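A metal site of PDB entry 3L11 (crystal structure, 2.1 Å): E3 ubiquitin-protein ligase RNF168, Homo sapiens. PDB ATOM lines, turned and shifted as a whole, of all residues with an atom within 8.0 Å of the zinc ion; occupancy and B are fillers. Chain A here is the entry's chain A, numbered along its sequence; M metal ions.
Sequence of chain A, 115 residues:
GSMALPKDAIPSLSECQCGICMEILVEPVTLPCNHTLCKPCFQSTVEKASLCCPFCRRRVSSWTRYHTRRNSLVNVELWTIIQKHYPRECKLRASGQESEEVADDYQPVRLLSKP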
ATOM      1  N   LEU A  31       5.170  -1.849   7.577  1.00  0.00           N
ATOM      2  CA  LEU A  31       4.959  -3.081   8.277  1.00  0.00           C
ATOM      3  C   LEU A  31       5.701  -2.981   9.590  1.00  0.00           C
ATOM      4  O   LEU A  31       6.505  -2.090   9.752  1.00  0.00           O
ATOM      5  CB  LEU A  31       5.484  -4.240   7.455  1.00  0.00           C
ATOM      6  CG  LEU A  31       4.694  -4.295   6.131  1.00  0.00           C
ATOM      7  CD1 LEU A  31       5.059  -5.518   5.262  1.00  0.00           C
ATOM      8  CD2 LEU A  31       3.217  -4.322   6.439  1.00  0.00           C
ATOM      9  N   PRO A  32       5.411  -3.883  10.558  1.00  0.00           N
ATOM     10  CA  PRO A  32       6.020  -3.625  11.856  1.00  0.00           C
ATOM     11  C   PRO A  32       7.521  -3.954  11.908  1.00  0.00           C
ATOM     12  O   PRO A  32       8.168  -3.524  12.844  1.00  0.00           O
ATOM     13  CB  PRO A  32       5.194  -4.485  12.832  1.00  0.00           C
ATOM     14  CG  PRO A  32       4.715  -5.632  11.982  1.00  0.00           C
ATOM     15  CD  PRO A  32       4.360  -4.912  10.624  1.00  0.00           C
ATOM     16  N   CYS A  33       8.034  -4.682  10.910  1.00  0.00           N
ATOM     17  CA  CYS A  33       9.433  -4.842  10.667  1.00  0.00           C
ATOM     18  C   CYS A  33      10.111  -3.577  10.039  1.00  0.00           C
ATOM     19  O   CYS A  33      11.278  -3.597   9.742  1.00  0.00           O
ATOM     20  CB  CYS A  33       9.575  -6.026   9.729  1.00  0.00           C
ATOM     21  SG  CYS A  33       8.637  -5.741   8.173  1.00  0.00           S
ATOM     22  N   ASN A  34       9.359  -2.480   9.910  1.00  0.00           N
ATOM     23  CA  ASN A  34       9.799  -1.213   9.334  1.00  0.00           C
ATOM     24  C   ASN A  34      10.052  -1.209   7.861  1.00  0.00           C
ATOM     25  O   ASN A  34      10.621  -0.265   7.389  1.00  0.00           O
ATOM     26  CB  ASN A  34      10.964  -0.583  10.069  1.00  0.00           C
ATOM     27  CG  ASN A  34      10.616  -0.349  11.464  1.00  0.00           C
ATOM     28  OD1 ASN A  34      11.209  -0.982  12.364  1.00  0.00           O
ATOM     29  ND2 ASN A  34       9.529   0.409  11.681  1.00  0.00           N
ATOM     30  N   HIS A  35       9.580  -2.210   7.132  1.00  0.00           N
ATOM     31  CA  HIS A  35       9.635  -2.101   5.673  1.00  0.00           C
ATOM     32  C   HIS A  35       8.356  -1.447   5.214  1.00  0.00           C
ATOM     33  O   HIS A  35       7.263  -1.681   5.759  1.00  0.00           O
ATOM     34  CB  HIS A  35       9.855  -3.464   5.062  1.00  0.00           C
ATOM     35  CG  HIS A  35      11.166  -4.067   5.451  1.00  0.00           C
ATOM     36  ND1 HIS A  35      11.281  -5.234   6.184  1.00  0.00           N
ATOM     37  CD2 HIS A  35      12.434  -3.639   5.228  1.00  0.00           C
ATOM     38  CE1 HIS A  35      12.552  -5.485   6.426  1.00  0.00           C
ATOM     39  NE2 HIS A  35      13.271  -4.526   5.879  1.00  0.00           N
ATOM     40  N   THR A  36       8.483  -0.645   4.178  1.00  0.00           N
ATOM     41  CA  THR A  36       7.367   0.090   3.646  1.00  0.00           C
ATOM     42  C   THR A  36       7.083  -0.284   2.190  1.00  0.00           C
ATOM     43  O   THR A  36       7.997  -0.612   1.434  1.00  0.00           O
ATOM     44  CB  THR A  36       7.647   1.581   3.805  1.00  0.00           C
ATOM     45  OG1 THR A  36       7.581   1.849   5.208  1.00  0.00           O
ATOM     46  CG2 THR A  36       6.557   2.380   3.248  1.00  0.00           C
ATOM     47  N   CYS A  52       2.854 -11.828   4.505  1.00  0.00           N
ATOM     48  CA  CYS A  52       4.253 -11.723   5.019  1.00  0.00           C
ATOM     49  C   CYS A  52       4.821 -10.460   4.373  1.00  0.00           C
ATOM     50  O   CYS A  52       4.443 -10.087   3.235  1.00  0.00           O
ATOM     51  CB  CYS A  52       5.119 -12.909   4.502  1.00  0.00           C
ATOM     52  SG  CYS A  52       4.478 -14.403   5.070  1.00  0.00           S
ATOM     53  N   CYS A  53       5.745  -9.825   5.069  1.00  0.00           N
ATOM     54  CA  CYS A  53       6.454  -8.708   4.500  1.00  0.00           C
ATOM     55  C   CYS A  53       7.181  -9.222   3.218  1.00  0.00           C
ATOM     56  O   CYS A  53       7.885 -10.261   3.248  1.00  0.00           O
ATOM     57  CB  CYS A  53       7.450  -8.150   5.514  1.00  0.00           C
ATOM     58  SG  CYS A  53       8.513  -6.876   4.746  1.00  0.00           S
ATOM     59  N   PRO A  54       6.982  -8.551   2.075  1.00  0.00           N
ATOM     60  CA  PRO A  54       7.731  -9.009   0.916  1.00  0.00           C
ATOM     61  C   PRO A  54       9.230  -8.755   0.962  1.00  0.00           C
ATOM     62  O   PRO A  54       9.889  -9.245   0.070  1.00  0.00           O
ATOM     63  CB  PRO A  54       7.122  -8.219  -0.265  1.00  0.00           C
ATOM     64  CG  PRO A  54       6.228  -7.261   0.299  1.00  0.00           C
ATOM     65  CD  PRO A  54       6.289  -7.271   1.810  1.00  0.00           C
ATOM     66  N   PHE A  55       9.734  -7.999   1.928  1.00  0.00           N
ATOM     67  CA  PHE A  55      11.168  -7.768   2.101  1.00  0.00           C
ATOM     68  C   PHE A  55      11.856  -8.726   3.063  1.00  0.00           C
ATOM     69  O   PHE A  55      12.979  -9.108   2.805  1.00  0.00           O
ATOM     70  CB  PHE A  55      11.501  -6.321   2.483  1.00  0.00           C
ATOM     71  CG  PHE A  55      10.901  -5.321   1.543  1.00  0.00           C
ATOM     72  CD1 PHE A  55      11.581  -4.880   0.425  1.00  0.00           C
ATOM     73  CD2 PHE A  55       9.613  -4.804   1.803  1.00  0.00           C
ATOM     74  CE1 PHE A  55      11.006  -3.937  -0.424  1.00  0.00           C
ATOM     75  CE2 PHE A  55       9.020  -3.867   0.930  1.00  0.00           C
ATOM     76  CZ  PHE A  55       9.747  -3.426  -0.172  1.00  0.00           C
ATOM     77  N   CYS A  56      11.202  -9.131   4.140  1.00  0.00           N
ATOM     78  CA  CYS A  56      11.883  -9.960   5.110  1.00  0.00           C
ATOM     79  C   CYS A  56      11.083 -11.160   5.515  1.00  0.00           C
ATOM     80  O   CYS A  56      11.543 -11.965   6.312  1.00  0.00           O
ATOM     81  CB  CYS A  56      12.270  -9.181   6.367  1.00  0.00           C
ATOM     82  SG  CYS A  56      10.786  -8.555   7.264  1.00  0.00           S
ATOM     83  N   ARG A  57       9.875 -11.282   4.983  1.00  0.00           N
ATOM     84  CA  ARG A  57       9.014 -12.493   5.250  1.00  0.00           C
ATOM     85  C   ARG A  57       8.478 -12.547   6.680  1.00  0.00           C
ATOM     86  O   ARG A  57       7.917 -13.566   7.153  1.00  0.00           O
ATOM     87  CB  ARG A  57       9.705 -13.793   4.939  1.00  0.00           C
ATOM     88  CG  ARG A  57      10.348 -13.915   3.551  1.00  0.00           C
ATOM     89  CD  ARG A  57       9.435 -13.577   2.363  1.00  0.00           C
ATOM     90  NE  ARG A  57       8.207 -14.385   2.367  1.00  0.00           N
ATOM     91  CZ  ARG A  57       7.196 -14.080   1.539  1.00  0.00           C
ATOM     92  NH1 ARG A  57       6.077 -14.813   1.580  1.00  0.00           N
ATOM     93  NH2 ARG A  57       7.307 -13.029   0.665  1.00  0.00           N
ATOM     94  N   ARG A  58       8.644 -11.456   7.383  1.00  0.00           N
ATOM     95  CA  ARG A  58       7.931 -11.303   8.648  1.00  0.00           C
ATOM     96  C   ARG A  58       6.393 -11.542   8.488  1.00  0.00           C
ATOM     97  O   ARG A  58       5.768 -10.904   7.619  1.00  0.00           O
ATOM     98  CB  ARG A  58       8.207  -9.880   9.108  1.00  0.00           C
ATOM     99  CG  ARG A  58       7.273  -9.259  10.100  1.00  0.00           C
ATOM    100  CD  ARG A  58       7.767  -9.535  11.406  1.00  0.00           C
ATOM    101  NE  ARG A  58       6.848  -9.129  12.479  1.00  0.00           N
ATOM    102  CZ  ARG A  58       7.169  -8.193  13.311  1.00  0.00           C
ATOM    103  NH1 ARG A  58       8.339  -7.601  13.084  1.00  0.00           N
ATOM    104  NH2 ARG A  58       6.360  -7.870  14.341  1.00  0.00           N
ATOM    105  N   ARG A  59       5.808 -12.390   9.337  1.00  0.00           N
ATOM    106  CA  ARG A  59       4.346 -12.664   9.285  1.00  0.00           C
ATOM    107  C   ARG A  59       3.646 -11.393   9.697  1.00  0.00           C
ATOM    108  O   ARG A  59       4.094 -10.739  10.646  1.00  0.00           O
ATOM    109  CB  ARG A  59       3.938 -13.811  10.209  1.00  0.00           C
ATOM    110  CG  ARG A  59       2.433 -14.193  10.229  1.00  0.00           C
ATOM    111  CD  ARG A  59       2.173 -14.928  11.503  1.00  0.00           C
ATOM    112  NE  ARG A  59       0.848 -15.464  11.743  1.00  0.00           N
ATOM    113  CZ  ARG A  59       0.067 -15.087  12.764  1.00  0.00           C
ATOM    114  NH1 ARG A  59      -1.140 -15.644  12.949  1.00  0.00           N
ATOM    115  NH2 ARG A  59       0.463 -14.156  13.605  1.00  0.00           N
ATOM    116  N   VAL A  60       2.573 -11.025   8.987  1.00  0.00           N
ATOM    117  CA  VAL A  60       1.862  -9.787   9.229  1.00  0.00           C
ATOM    118  C   VAL A  60       0.310  -9.935   9.149  1.00  0.00           C
ATOM    119  O   VAL A  60      -0.445  -8.972   8.940  1.00  0.00           O
ATOM    120  CB  VAL A  60       2.543  -8.839   8.200  1.00  0.00           C
ATOM    121  CG1 VAL A  60       1.815  -8.534   6.939  1.00  0.00           C
ATOM    122  CG2 VAL A  60       3.586  -7.910   8.828  1.00  0.00           C
HETATM  123 ZN    ZN M   1       9.856  -6.639   6.558  1.00  0.00          ZN
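Along chain A the residues within 4 Å of the zinc ion span positions 33 to 56.
The side-chain sulfur (SG) of Cys 56 lies close to the backbone NH (N) of Arg 58 (3.6 Å).
The backbone NH of Phe 55 sits close to the side-chain sulfur of Cys 53 (3.3 Å).
The backbone carbonyl oxygen (O) of Arg 58 is in hydrogen-bond range of the backbone NH (N) of Cys 53.
The zinc ion is bound by ND1 of His 35.
The side-chain sulfur (SG) of Cys 33 is bound to the zinc ion (2.2 Å).
The side-chain sulfur (SG) of Cys 56 binds the zinc ion (2.2 Å).
The zinc ion is bound by the side-chain sulfur (SG) of Cys 53, 2.3 Å away.
The zinc ion has four donor atoms within binding distance.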
